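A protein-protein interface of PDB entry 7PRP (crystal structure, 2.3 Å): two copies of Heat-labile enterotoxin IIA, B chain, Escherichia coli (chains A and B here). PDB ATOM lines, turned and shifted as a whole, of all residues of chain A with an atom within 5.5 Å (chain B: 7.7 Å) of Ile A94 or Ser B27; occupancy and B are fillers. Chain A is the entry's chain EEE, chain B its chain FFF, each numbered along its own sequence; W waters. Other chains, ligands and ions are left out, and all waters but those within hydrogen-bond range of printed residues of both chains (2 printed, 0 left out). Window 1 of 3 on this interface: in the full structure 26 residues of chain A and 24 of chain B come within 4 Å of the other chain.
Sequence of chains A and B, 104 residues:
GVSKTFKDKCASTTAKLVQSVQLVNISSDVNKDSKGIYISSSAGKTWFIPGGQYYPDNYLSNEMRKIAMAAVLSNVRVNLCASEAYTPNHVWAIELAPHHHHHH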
ATOM      1  N   PHE A   6      18.693   0.803   9.544  1.00  0.00           N
ATOM      2  CA  PHE A   6      18.978   1.310   8.185  1.00  0.00           C
ATOM      3  C   PHE A   6      17.712   1.211   7.327  1.00  0.00           C
ATOM      4  O   PHE A   6      17.403   2.185   6.655  1.00  0.00           O
ATOM      5  CB  PHE A   6      20.140   0.575   7.516  1.00  0.00           C
ATOM      6  CG  PHE A   6      20.681   1.295   6.309  1.00  0.00           C
ATOM      7  CD1 PHE A   6      21.571   2.357   6.433  1.00  0.00           C
ATOM      8  CD2 PHE A   6      20.254   0.944   5.040  1.00  0.00           C
ATOM      9  CE1 PHE A   6      22.046   3.007   5.312  1.00  0.00           C
ATOM     10  CE2 PHE A   6      20.715   1.623   3.922  1.00  0.00           C
ATOM     11  CZ  PHE A   6      21.622   2.630   4.058  1.00  0.00           C
ATOM     12  N   LEU A  23      30.277  -3.057  -4.560  1.00  0.00           N
ATOM     13  CA  LEU A  23      30.895  -1.955  -5.314  1.00  0.00           C
ATOM     14  C   LEU A  23      32.215  -2.461  -5.887  1.00  0.00           C
ATOM     15  O   LEU A  23      32.949  -3.121  -5.157  1.00  0.00           O
ATOM     16  CB  LEU A  23      31.071  -0.754  -4.386  1.00  0.00           C
ATOM     17  CG  LEU A  23      29.788  -0.106  -3.876  1.00  0.00           C
ATOM     18  CD1 LEU A  23      30.133   1.031  -2.929  1.00  0.00           C
ATOM     19  CD2 LEU A  23      28.873   0.367  -5.004  1.00  0.00           C
ATOM     20  N   ILE A  39      30.267   5.891  -7.552  1.00  0.00           N
ATOM     21  CA  ILE A  39      30.474   4.454  -7.212  1.00  0.00           C
ATOM     22  C   ILE A  39      29.629   3.593  -8.153  1.00  0.00           C
ATOM     23  O   ILE A  39      28.474   3.992  -8.507  1.00  0.00           O
ATOM     24  CB  ILE A  39      30.112   4.193  -5.746  1.00  0.00           C
ATOM     25  CG1 ILE A  39      28.678   4.626  -5.417  1.00  0.00           C
ATOM     26  CG2 ILE A  39      31.174   4.871  -4.883  1.00  0.00           C
ATOM     27  CD1 ILE A  39      28.165   4.146  -4.088  1.00  0.00           C
ATOM     28  N   ILE A  49      27.654  10.208  -4.799  1.00  0.00           N
ATOM     29  CA  ILE A  49      27.713  10.545  -3.354  1.00  0.00           C
ATOM     30  C   ILE A  49      27.869  12.054  -3.226  1.00  0.00           C
ATOM     31  O   ILE A  49      28.907  12.635  -3.541  1.00  0.00           O
ATOM     32  CB  ILE A  49      28.852   9.816  -2.632  1.00  0.00           C
ATOM     33  CG1 ILE A  49      28.768   8.322  -2.843  1.00  0.00           C
ATOM     34  CG2 ILE A  49      28.830  10.149  -1.161  1.00  0.00           C
ATOM     35  CD1 ILE A  49      29.867   7.539  -2.184  1.00  0.00           C
ATOM     36  N   GLU A  63      32.344  10.269   5.920  1.00  0.00           N
ATOM     37  CA  GLU A  63      32.180   8.860   6.372  1.00  0.00           C
ATOM     38  C   GLU A  63      31.534   8.039   5.247  1.00  0.00           C
ATOM     39  O   GLU A  63      31.949   6.895   5.071  1.00  0.00           O
ATOM     40  CB  GLU A  63      31.399   8.730   7.682  1.00  0.00           C
ATOM     41  CG  GLU A  63      32.132   9.344   8.845  1.00  0.00           C
ATOM     42  CD  GLU A  63      33.448   8.663   9.254  1.00  0.00           C
ATOM     43  OE1 GLU A  63      33.611   7.385   9.070  1.00  0.00           O
ATOM     44  OE2 GLU A  63      34.296   9.395   9.846  1.00  0.00           O
ATOM     45  N   MET A  64      30.583   8.594   4.491  1.00  0.00           N
ATOM     46  CA  MET A  64      29.983   7.874   3.336  1.00  0.00           C
ATOM     47  C   MET A  64      31.096   7.490   2.353  1.00  0.00           C
ATOM     48  O   MET A  64      31.151   6.322   1.958  1.00  0.00           O
ATOM     49  CB  MET A  64      28.923   8.710   2.644  1.00  0.00           C
ATOM     50  CG  MET A  64      27.676   8.954   3.509  1.00  0.00           C
ATOM     51  SD  MET A  64      26.376   9.790   2.502  1.00  0.00           S
ATOM     52  CE  MET A  64      25.813   8.469   1.490  1.00  0.00           C
ATOM     53  N   ILE A  67      33.342   4.665   3.768  1.00  0.00           N
ATOM     54  CA  ILE A  67      32.615   3.360   3.703  1.00  0.00           C
ATOM     55  C   ILE A  67      32.681   2.822   2.265  1.00  0.00           C
ATOM     56  O   ILE A  67      33.041   1.650   2.096  1.00  0.00           O
ATOM     57  CB  ILE A  67      31.183   3.509   4.238  1.00  0.00           C
ATOM     58  CG1 ILE A  67      31.209   3.740   5.745  1.00  0.00           C
ATOM     59  CG2 ILE A  67      30.326   2.308   3.892  1.00  0.00           C
ATOM     60  CD1 ILE A  67      29.873   4.221   6.305  1.00  0.00           C
ATOM     61  N   ALA A  68      32.331   3.637   1.269  1.00  0.00           N
ATOM     62  CA  ALA A  68      32.331   3.212  -0.158  1.00  0.00           C
ATOM     63  C   ALA A  68      33.738   2.766  -0.579  1.00  0.00           C
ATOM     64  O   ALA A  68      33.865   1.782  -1.246  1.00  0.00           O
ATOM     65  CB  ALA A  68      31.835   4.347  -1.011  1.00  0.00           C
ATOM     66  N   VAL A  78      27.772  -3.291   0.645  1.00  0.00           N
ATOM     67  CA  VAL A  78      27.098  -2.139   1.289  1.00  0.00           C
ATOM     68  C   VAL A  78      25.571  -2.253   1.099  1.00  0.00           C
ATOM     69  O   VAL A  78      25.116  -2.940   0.146  1.00  0.00           O
ATOM     70  CB  VAL A  78      27.620  -0.794   0.739  1.00  0.00           C
ATOM     71  CG1 VAL A  78      29.100  -0.618   0.984  1.00  0.00           C
ATOM     72  CG2 VAL A  78      27.304  -0.577  -0.729  1.00  0.00           C
ATOM     73  N   ASN A  79      24.817  -1.524   1.921  1.00  0.00           N
ATOM     74  CA  ASN A  79      23.400  -1.212   1.632  1.00  0.00           C
ATOM     75  C   ASN A  79      23.329   0.285   1.354  1.00  0.00           C
ATOM     76  O   ASN A  79      24.136   1.006   1.972  1.00  0.00           O
ATOM     77  CB  ASN A  79      22.457  -1.657   2.750  1.00  0.00           C
ATOM     78  CG  ASN A  79      22.769  -3.043   3.227  1.00  0.00           C
ATOM     79  OD1 ASN A  79      22.667  -3.973   2.463  1.00  0.00           O
ATOM     80  ND2 ASN A  79      23.155  -3.189   4.490  1.00  0.00           N
ATOM     81  N   LEU A  80      22.465   0.705   0.429  1.00  0.00           N
ATOM     82  CA  LEU A  80      22.318   2.131   0.039  1.00  0.00           C
ATOM     83  C   LEU A  80      20.878   2.594   0.248  1.00  0.00           C
ATOM     84  O   LEU A  80      19.935   1.805   0.052  1.00  0.00           O
ATOM     85  CB  LEU A  80      22.689   2.339  -1.443  1.00  0.00           C
ATOM     86  CG  LEU A  80      24.124   1.993  -1.798  1.00  0.00           C
ATOM     87  CD1 LEU A  80      24.315   2.042  -3.256  1.00  0.00           C
ATOM     88  CD2 LEU A  80      25.088   2.928  -1.118  1.00  0.00           C
ATOM     89  N   CYS A  81      20.750   3.872   0.581  1.00  0.00           N
ATOM     90  CA  CYS A  81      19.503   4.649   0.519  1.00  0.00           C
ATOM     91  C   CYS A  81      19.726   5.673  -0.592  1.00  0.00           C
ATOM     92  O   CYS A  81      20.546   6.559  -0.390  1.00  0.00           O
ATOM     93  CB  CYS A  81      19.207   5.297   1.860  1.00  0.00           C
ATOM     94  SG  CYS A  81      17.528   5.979   1.939  1.00  0.00           S
ATOM     95  N   VAL A  91      23.165   8.990  -3.386  1.00  0.00           N
ATOM     96  CA  VAL A  91      23.224   8.296  -2.079  1.00  0.00           C
ATOM     97  C   VAL A  91      22.989   9.286  -0.940  1.00  0.00           C
ATOM     98  O   VAL A  91      23.783  10.224  -0.765  1.00  0.00           O
ATOM     99  CB  VAL A  91      24.561   7.578  -1.898  1.00  0.00           C
ATOM    100  CG1 VAL A  91      24.552   6.766  -0.624  1.00  0.00           C
ATOM    101  CG2 VAL A  91      24.913   6.699  -3.080  1.00  0.00           C
ATOM    102  N   TRP A  92      21.959   9.020  -0.135  1.00  0.00           N
ATOM    103  CA  TRP A  92      21.608   9.764   1.092  1.00  0.00           C
ATOM    104  C   TRP A  92      21.950   8.953   2.349  1.00  0.00           C
ATOM    105  O   TRP A  92      21.920   9.545   3.480  1.00  0.00           O
ATOM    106  CB  TRP A  92      20.128  10.166   1.025  1.00  0.00           C
ATOM    107  CG  TRP A  92      19.848  11.232   0.009  1.00  0.00           C
ATOM    108  CD1 TRP A  92      20.747  12.017  -0.658  1.00  0.00           C
ATOM    109  CD2 TRP A  92      18.554  11.676  -0.415  1.00  0.00           C
ATOM    110  NE1 TRP A  92      20.100  12.870  -1.521  1.00  0.00           N
ATOM    111  CE2 TRP A  92      18.753  12.714  -1.351  1.00  0.00           C
ATOM    112  CE3 TRP A  92      17.247  11.313  -0.076  1.00  0.00           C
ATOM    113  CZ2 TRP A  92      17.686  13.393  -1.938  1.00  0.00           C
ATOM    114  CZ3 TRP A  92      16.195  11.953  -0.695  1.00  0.00           C
ATOM    115  CH2 TRP A  92      16.414  12.986  -1.603  1.00  0.00           C
ATOM    116  N   ALA A  93      22.250   7.656   2.219  1.00  0.00           N
ATOM    117  CA  ALA A  93      22.867   6.908   3.330  1.00  0.00           C
ATOM    118  C   ALA A  93      23.576   5.701   2.750  1.00  0.00           C
ATOM    119  O   ALA A  93      23.091   5.164   1.760  1.00  0.00           O
ATOM    120  CB  ALA A  93      21.823   6.494   4.338  1.00  0.00           C
ATOM    121  N   ILE A  94      24.601   5.228   3.433  1.00  0.00           N
ATOM    122  CA  ILE A  94      25.327   3.999   3.048  1.00  0.00           C
ATOM    123  C   ILE A  94      25.679   3.232   4.321  1.00  0.00           C
ATOM    124  O   ILE A  94      26.019   3.838   5.328  1.00  0.00           O
ATOM    125  CB  ILE A  94      26.563   4.340   2.184  1.00  0.00           C
ATOM    126  CG1 ILE A  94      27.210   3.072   1.598  1.00  0.00           C
ATOM    127  CG2 ILE A  94      27.553   5.177   2.971  1.00  0.00           C
ATOM    128  CD1 ILE A  94      28.217   3.356   0.544  1.00  0.00           C
ATOM    129  N   GLU A  95      25.565   1.913   4.278  1.00  0.00           N
ATOM    130  CA  GLU A  95      25.889   1.028   5.420  1.00  0.00           C
ATOM    131  C   GLU A  95      26.903  -0.013   4.945  1.00  0.00           C
ATOM    132  O   GLU A  95      26.664  -0.693   3.908  1.00  0.00           O
ATOM    133  CB  GLU A  95      24.598   0.379   5.910  1.00  0.00           C
ATOM    134  CG  GLU A  95      24.801  -0.660   6.992  1.00  0.00           C
ATOM    135  CD  GLU A  95      23.518  -1.085   7.674  1.00  0.00           C
ATOM    136  OE1 GLU A  95      23.221  -0.501   8.748  1.00  0.00           O
ATOM    137  OE2 GLU A  95      22.768  -1.876   7.099  1.00  0.00           O
ATOM    138  N   LEU A  96      28.018  -0.109   5.646  1.00  0.00           N
ATOM    139  CA  LEU A  96      29.012  -1.176   5.423  1.00  0.00           C
ATOM    140  C   LEU A  96      28.405  -2.460   5.963  1.00  0.00           C
ATOM    141  O   LEU A  96      27.958  -2.430   7.145  1.00  0.00           O
ATOM    142  CB  LEU A  96      30.302  -0.797   6.143  1.00  0.00           C
ATOM    143  CG  LEU A  96      31.497  -1.661   5.795  1.00  0.00           C
ATOM    144  CD1 LEU A  96      31.874  -1.464   4.356  1.00  0.00           C
ATOM    145  CD2 LEU A  96      32.659  -1.414   6.723  1.00  0.00           C
ATOM    146  N   ASN B  25      27.572  -3.688  11.269  1.00  0.00           N
ATOM    147  CA  ASN B  25      27.158  -2.601  10.361  1.00  0.00           C
ATOM    148  C   ASN B  25      27.597  -1.259  10.927  1.00  0.00           C
ATOM    149  O   ASN B  25      27.488  -1.033  12.166  1.00  0.00           O
ATOM    150  CB  ASN B  25      25.651  -2.557  10.130  1.00  0.00           C
ATOM    151  CG  ASN B  25      25.097  -3.768   9.414  1.00  0.00           C
ATOM    152  OD1 ASN B  25      24.326  -4.512  10.008  1.00  0.00           O
ATOM    153  ND2 ASN B  25      25.495  -3.977   8.159  1.00  0.00           N
ATOM    154  N   ILE B  26      28.108  -0.398  10.046  1.00  0.00           N
ATOM    155  CA  ILE B  26      28.266   1.052  10.341  1.00  0.00           C
ATOM    156  C   ILE B  26      27.600   1.784   9.186  1.00  0.00           C
ATOM    157  O   ILE B  26      27.780   1.413   8.013  1.00  0.00           O
ATOM    158  CB  ILE B  26      29.741   1.428  10.605  1.00  0.00           C
ATOM    159  CG1 ILE B  26      29.887   2.898  10.964  1.00  0.00           C
ATOM    160  CG2 ILE B  26      30.665   1.043   9.451  1.00  0.00           C
ATOM    161  CD1 ILE B  26      31.191   3.212  11.733  1.00  0.00           C
ATOM    162  N   SER B  27      26.872   2.835   9.502  1.00  0.00           N
ATOM    163  CA  SER B  27      26.170   3.646   8.480  1.00  0.00           C
ATOM    164  C   SER B  27      26.407   5.142   8.750  1.00  0.00           C
ATOM    165  O   SER B  27      26.580   5.546   9.903  1.00  0.00           O
ATOM    166  CB  SER B  27      24.714   3.273   8.445  1.00  0.00           C
ATOM    167  OG  SER B  27      24.066   3.627   9.678  1.00  0.00           O
ATOM    168  N   SER B  28      26.465   5.907   7.672  1.00  0.00           N
ATOM    169  CA  SER B  28      26.458   7.359   7.620  1.00  0.00           C
ATOM    170  C   SER B  28      25.257   7.796   6.790  1.00  0.00           C
ATOM    171  O   SER B  28      25.066   7.239   5.716  1.00  0.00           O
ATOM    172  CB  SER B  28      27.751   7.870   7.086  1.00  0.00           C
ATOM    173  OG  SER B  28      27.750   9.290   7.219  1.00  0.00           O
ATOM    174  N   ASP B  29      24.474   8.733   7.299  1.00  0.00           N
ATOM    175  CA  ASP B  29      23.133   9.126   6.792  1.00  0.00           C
ATOM    176  C   ASP B  29      23.080  10.653   6.679  1.00  0.00           C
ATOM    177  O   ASP B  29      23.365  11.292   7.675  1.00  0.00           O
ATOM    178  CB  ASP B  29      22.055   8.587   7.743  1.00  0.00           C
ATOM    179  CG  ASP B  29      20.623   8.679   7.215  1.00  0.00           C
ATOM    180  OD1 ASP B  29      20.335   9.583   6.403  1.00  0.00           O
ATOM    181  OD2 ASP B  29      19.782   7.871   7.667  1.00  0.00           O
ATOM    182  N   VAL B  30      22.742  11.219   5.514  1.00  0.00           N
ATOM    183  CA  VAL B  30      22.567  12.698   5.350  1.00  0.00           C
ATOM    184  C   VAL B  30      21.098  13.047   5.032  1.00  0.00           C
ATOM    185  O   VAL B  30      20.872  14.129   4.583  1.00  0.00           O
ATOM    186  CB  VAL B  30      23.538  13.265   4.298  1.00  0.00           C
ATOM    187  CG1 VAL B  30      24.994  13.053   4.730  1.00  0.00           C
ATOM    188  CG2 VAL B  30      23.266  12.695   2.904  1.00  0.00           C
ATOM    189  N   ASN B  31      20.143  12.145   5.264  1.00  0.00           N
ATOM    190  CA  ASN B  31      18.690  12.439   5.142  1.00  0.00           C
ATOM    191  C   ASN B  31      18.265  13.464   6.161  1.00  0.00           C
ATOM    192  O   ASN B  31      18.701  13.304   7.304  1.00  0.00           O
ATOM    193  CB  ASN B  31      17.829  11.204   5.386  1.00  0.00           C
ATOM    194  CG  ASN B  31      17.724  10.397   4.127  1.00  0.00           C
ATOM    195  OD1 ASN B  31      17.139  10.902   3.159  1.00  0.00           O
ATOM    196  ND2 ASN B  31      18.288   9.192   4.139  1.00  0.00           N
ATOM    197  N   SER B  34      17.120  12.034   9.636  1.00  0.00           N
ATOM    198  CA  SER B  34      17.751  10.767  10.076  1.00  0.00           C
ATOM    199  C   SER B  34      19.280  10.921  10.144  1.00  0.00           C
ATOM    200  O   SER B  34      19.929   9.927  10.374  1.00  0.00           O
ATOM    201  CB  SER B  34      17.318   9.606   9.192  1.00  0.00           C
ATOM    202  OG  SER B  34      16.510   9.948   8.052  1.00  0.00           O
ATOM    203  N   GLY B  36      23.186  11.160  10.752  1.00  0.00           N
ATOM    204  CA  GLY B  36      24.129  10.734  11.820  1.00  0.00           C
ATOM    205  C   GLY B  36      24.844   9.416  11.521  1.00  0.00           C
ATOM    206  O   GLY B  36      24.651   8.831  10.403  1.00  0.00           O
ATOM    207  N   ILE B  37      25.637   8.966  12.487  1.00  0.00           N
ATOM    208  CA  ILE B  37      26.388   7.685  12.417  1.00  0.00           C
ATOM    209  C   ILE B  37      25.704   6.674  13.311  1.00  0.00           C
ATOM    210  O   ILE B  37      25.477   6.966  14.504  1.00  0.00           O
ATOM    211  CB  ILE B  37      27.837   7.903  12.854  1.00  0.00           C
ATOM    212  CG1 ILE B  37      28.498   9.007  12.022  1.00  0.00           C
ATOM    213  CG2 ILE B  37      28.592   6.599  12.784  1.00  0.00           C
ATOM    214  CD1 ILE B  37      28.642   8.657  10.559  1.00  0.00           C
ATOM    215  N   TYR B  38      25.386   5.537  12.744  1.00  0.00           N
ATOM    216  CA  TYR B  38      24.703   4.421  13.456  1.00  0.00           C
ATOM    217  C   TYR B  38      25.605   3.186  13.325  1.00  0.00           C
ATOM    218  O   TYR B  38      26.244   2.990  12.258  1.00  0.00           O
ATOM    219  CB  TYR B  38      23.270   4.205  12.922  1.00  0.00           C
ATOM    220  CG  TYR B  38      22.353   5.412  13.016  1.00  0.00           C
ATOM    221  CD1 TYR B  38      22.297   6.357  11.997  1.00  0.00           C
ATOM    222  CD2 TYR B  38      21.591   5.655  14.159  1.00  0.00           C
ATOM    223  CE1 TYR B  38      21.468   7.463  12.073  1.00  0.00           C
ATOM    224  CE2 TYR B  38      20.769   6.760  14.254  1.00  0.00           C
ATOM    225  CZ  TYR B  38      20.694   7.670  13.209  1.00  0.00           C
ATOM    226  OH  TYR B  38      19.873   8.769  13.318  1.00  0.00           O
ATOM    227  N   ILE B  39      25.664   2.390  14.388  1.00  0.00           N
ATOM    228  CA  ILE B  39      26.373   1.092  14.458  1.00  0.00           C
ATOM    229  C   ILE B  39      25.433   0.028  15.023  1.00  0.00           C
ATOM    230  O   ILE B  39      24.645   0.329  15.946  1.00  0.00           O
ATOM    231  CB  ILE B  39      27.660   1.244  15.273  1.00  0.00           C
ATOM    232  CG1 ILE B  39      27.395   1.767  16.683  1.00  0.00           C
ATOM    233  CG2 ILE B  39      28.650   2.081  14.489  1.00  0.00           C
ATOM    234  CD1 ILE B  39      28.543   1.624  17.641  1.00  0.00           C
ATOM    235  N   SER B  40      25.526  -1.177  14.482  1.00  0.00           N
ATOM    236  CA  SER B  40      24.650  -2.311  14.862  1.00  0.00           C
ATOM    237  C   SER B  40      25.492  -3.551  15.162  1.00  0.00           C
ATOM    238  O   SER B  40      26.443  -3.804  14.431  1.00  0.00           O
ATOM    239  CB  SER B  40      23.606  -2.547  13.803  1.00  0.00           C
ATOM    240  OG  SER B  40      22.637  -1.494  13.823  1.00  0.00           O
ATOM    241  N   THR B  46      21.325  -1.393  18.050  1.00  0.00           N
ATOM    242  CA  THR B  46      21.837  -0.229  17.324  1.00  0.00           C
ATOM    243  C   THR B  46      22.223   0.851  18.347  1.00  0.00           C
ATOM    244  O   THR B  46      21.516   1.028  19.346  1.00  0.00           O
ATOM    245  CB  THR B  46      20.827   0.241  16.269  1.00  0.00           C
ATOM    246  OG1 THR B  46      20.595  -0.805  15.323  1.00  0.00           O
ATOM    247  CG2 THR B  46      21.335   1.420  15.472  1.00  0.00           C
ATOM    248  N   TRP B  47      23.300   1.573  18.075  1.00  0.00           N
ATOM    249  CA  TRP B  47      23.670   2.824  18.789  1.00  0.00           C
ATOM    250  C   TRP B  47      23.858   3.957  17.795  1.00  0.00           C
ATOM    251  O   TRP B  47      24.096   3.699  16.638  1.00  0.00           O
ATOM    252  CB  TRP B  47      24.935   2.646  19.648  1.00  0.00           C
ATOM    253  CG  TRP B  47      24.886   1.540  20.657  1.00  0.00           C
ATOM    254  CD1 TRP B  47      24.685   1.707  21.992  1.00  0.00           C
ATOM    255  CD2 TRP B  47      25.118   0.143  20.463  1.00  0.00           C
ATOM    256  NE1 TRP B  47      24.695   0.504  22.627  1.00  0.00           N
ATOM    257  CE2 TRP B  47      24.967  -0.479  21.722  1.00  0.00           C
ATOM    258  CE3 TRP B  47      25.383  -0.665  19.358  1.00  0.00           C
ATOM    259  CZ2 TRP B  47      25.098  -1.854  21.912  1.00  0.00           C
ATOM    260  CZ3 TRP B  47      25.511  -2.024  19.541  1.00  0.00           C
ATOM    261  CH2 TRP B  47      25.368  -2.613  20.799  1.00  0.00           C
ATOM    262  N   ILE B  49      26.288   7.301  17.271  1.00  0.00           N
ATOM    263  CA  ILE B  49      27.550   7.983  17.646  1.00  0.00           C
ATOM    264  C   ILE B  49      27.372   9.479  17.413  1.00  0.00           C
ATOM    265  O   ILE B  49      27.267   9.936  16.281  1.00  0.00           O
ATOM    266  CB  ILE B  49      28.747   7.456  16.870  1.00  0.00           C
ATOM    267  CG1 ILE B  49      28.845   5.936  16.930  1.00  0.00           C
ATOM    268  CG2 ILE B  49      30.008   8.164  17.345  1.00  0.00           C
ATOM    269  CD1 ILE B  49      30.115   5.392  16.290  1.00  0.00           C
ATOM    270  N   ARG B  65      34.407   7.246  15.498  1.00  0.00           N
ATOM    271  CA  ARG B  65      33.984   6.713  14.169  1.00  0.00           C
ATOM    272  C   ARG B  65      35.079   5.795  13.592  1.00  0.00           C
ATOM    273  O   ARG B  65      34.735   4.691  13.088  1.00  0.00           O
ATOM    274  CB  ARG B  65      33.628   7.876  13.223  1.00  0.00           C
ATOM    275  CG  ARG B  65      32.462   8.697  13.725  1.00  0.00           C
ATOM    276  CD  ARG B  65      31.983   9.665  12.690  1.00  0.00           C
ATOM    277  NE  ARG B  65      32.977  10.650  12.269  1.00  0.00           N
ATOM    278  CZ  ARG B  65      33.107  11.872  12.791  1.00  0.00           C
ATOM    279  NH1 ARG B  65      34.027  12.694  12.311  1.00  0.00           N
ATOM    280  NH2 ARG B  65      32.305  12.276  13.762  1.00  0.00           N
ATOM    281  N   MET B  69      34.532   1.866  12.758  1.00  0.00           N
ATOM    282  CA  MET B  69      34.727   1.461  11.345  1.00  0.00           C
ATOM    283  C   MET B  69      35.717   0.293  11.270  1.00  0.00           C
ATOM    284  O   MET B  69      35.422  -0.722  10.614  1.00  0.00           O
ATOM    285  CB  MET B  69      35.252   2.655  10.561  1.00  0.00           C
ATOM    286  CG  MET B  69      35.685   2.305   9.155  1.00  0.00           C
ATOM    287  SD  MET B  69      34.375   2.549   7.945  1.00  0.00           S
ATOM    288  CE  MET B  69      34.155   4.316   8.137  1.00  0.00           C
ATOM    289  N   VAL B  72      34.135  -2.977  12.423  1.00  0.00           N
ATOM    290  CA  VAL B  72      33.247  -3.627  11.422  1.00  0.00           C
ATOM    291  C   VAL B  72      34.105  -4.245  10.330  1.00  0.00           C
ATOM    292  O   VAL B  72      33.917  -5.399  10.021  1.00  0.00           O
ATOM    293  CB  VAL B  72      32.206  -2.649  10.856  1.00  0.00           C
ATOM    294  CG1 VAL B  72      31.385  -3.302   9.747  1.00  0.00           C
ATOM    295  CG2 VAL B  72      31.280  -2.119  11.970  1.00  0.00           C
HETATM  296  O   HOH W   1      24.532   0.610  10.861  1.00  0.00           O
HETATM  297  O   HOH W   2      35.957   6.219  10.311  1.00  0.00           O
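The side-chain carboxylate (OE2) of Glu A63 lies within salt-bridge range of the guanidinium group (NE) of Arg B65, 3.0 Å away. N of Leu A96 is in hydrogen-bond range of O of Ile B26, 2.8 Å away. The backbone NH (N) of Ile A94 is in hydrogen-bond range of the backbone carbonyl oxygen (O) of Ser B28, at 3.1 Å. O of Trp A92 lies within hydrogen-bond range of N of Val B30, at 2.8 Å. The side-chain amide nitrogen of Asn B25 lies within hydrogen-bond range of the backbone carbonyl oxygen of Leu A96. O of Trp A92 lies close to OD1 of Asp B29 (3.3 Å).
The backbone carbonyl oxygen of Ala A93 sits at hydrogen-bond distance from the backbone NH of Cys A81, at 2.9 Å. The backbone carbonyl oxygen (O) of Tyr B38 sits at hydrogen-bond distance from the backbone NH (N) of Ser B27, at 2.8 Å. The backbone carbonyl oxygen of Cys A81 is in hydrogen-bond range of the backbone NH of Trp A92. The backbone NH (N) of Asn A79 lies within hydrogen-bond range of the backbone carbonyl oxygen (O) of Glu A95 (2.8 Å). N of Ser B40 lies within hydrogen-bond range of O of Asn B25, 3.0 Å away. O of Asp B29 sits at hydrogen-bond distance from N of Gly B36, at 3.1 Å.
CB of Ser B27 touches CD1 of Phe A6, 3.8 Å away. Glu A63 touches Ser B28. Met A64 touches Ser B28. Met B69 touches Ile A67 (CE to CG1, 3.8 Å). Asn B31 touches Cys A81 (ND2 to SG, 3.97 Å). Asn B31 touches Trp A92 (OD1 to CE3, 3.3 Å). Ala A93 touches Ser B28 (CA to O, 3.3 Å). Asp B29 touches Ala A93 (CG to CB, 3.8 Å). OE1 of Glu A95 touches CB of Asn B25, 3.5 Å away. Val B72 touches Leu A96.
Of the printed residues of chain B, Ile A94 touches Ser B27 (3.2 Å) and Ser B28 (3.1 Å). Of chain A, only Phe A6, Ile A94 and Glu A95 come within 4 Å of Ser B27. Printed residues of chain B within 4 Å of Cys A81: Asn B31. Of the printed residues of chain A, Val B72 touches Leu A96 (3.8 Å). Of the printed residues of chain A, Arg B65 touches Glu A63. Printed residues of chain B within 4 Å of Phe A6: Ser B27. Of the printed residues of chain B, Leu A96 touches Asn B25 (3.1 Å), Ile B26 (2.8 Å) and Val B72 (3.8 Å). The nearest residue of chain B that does not touch Ile A94 is Ile B26 (4.02 Å).
Of the 18 printed residues of chain A, 10 touch a printed residue of chain B. Hydrophobic or aromatic side chains of chain A that line the printed part of chain B: Phe A6, Met A64, Ile A67, Trp A92, Ala A93 and Leu A96. Among the printed residues, Asp or Glu carboxylates within 4 Å of a Lys or Arg side-chain nitrogen of the other chain: Glu A63 with Arg B65 (3.0 Å).
2 positions are printed for both chains. Of the 22 pairs that touch across the chains among the printed residues, none has its exchanged pair printed and touching as well.
Water W1 lies within hydrogen-bond range of OE1 of Glu A95, O of Tyr B38 and OG of Ser B27. Water W2 bridges the side-chain carboxylate (OE1) of Glu A63 and the backbone carbonyl oxygen (O) of Arg B65.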
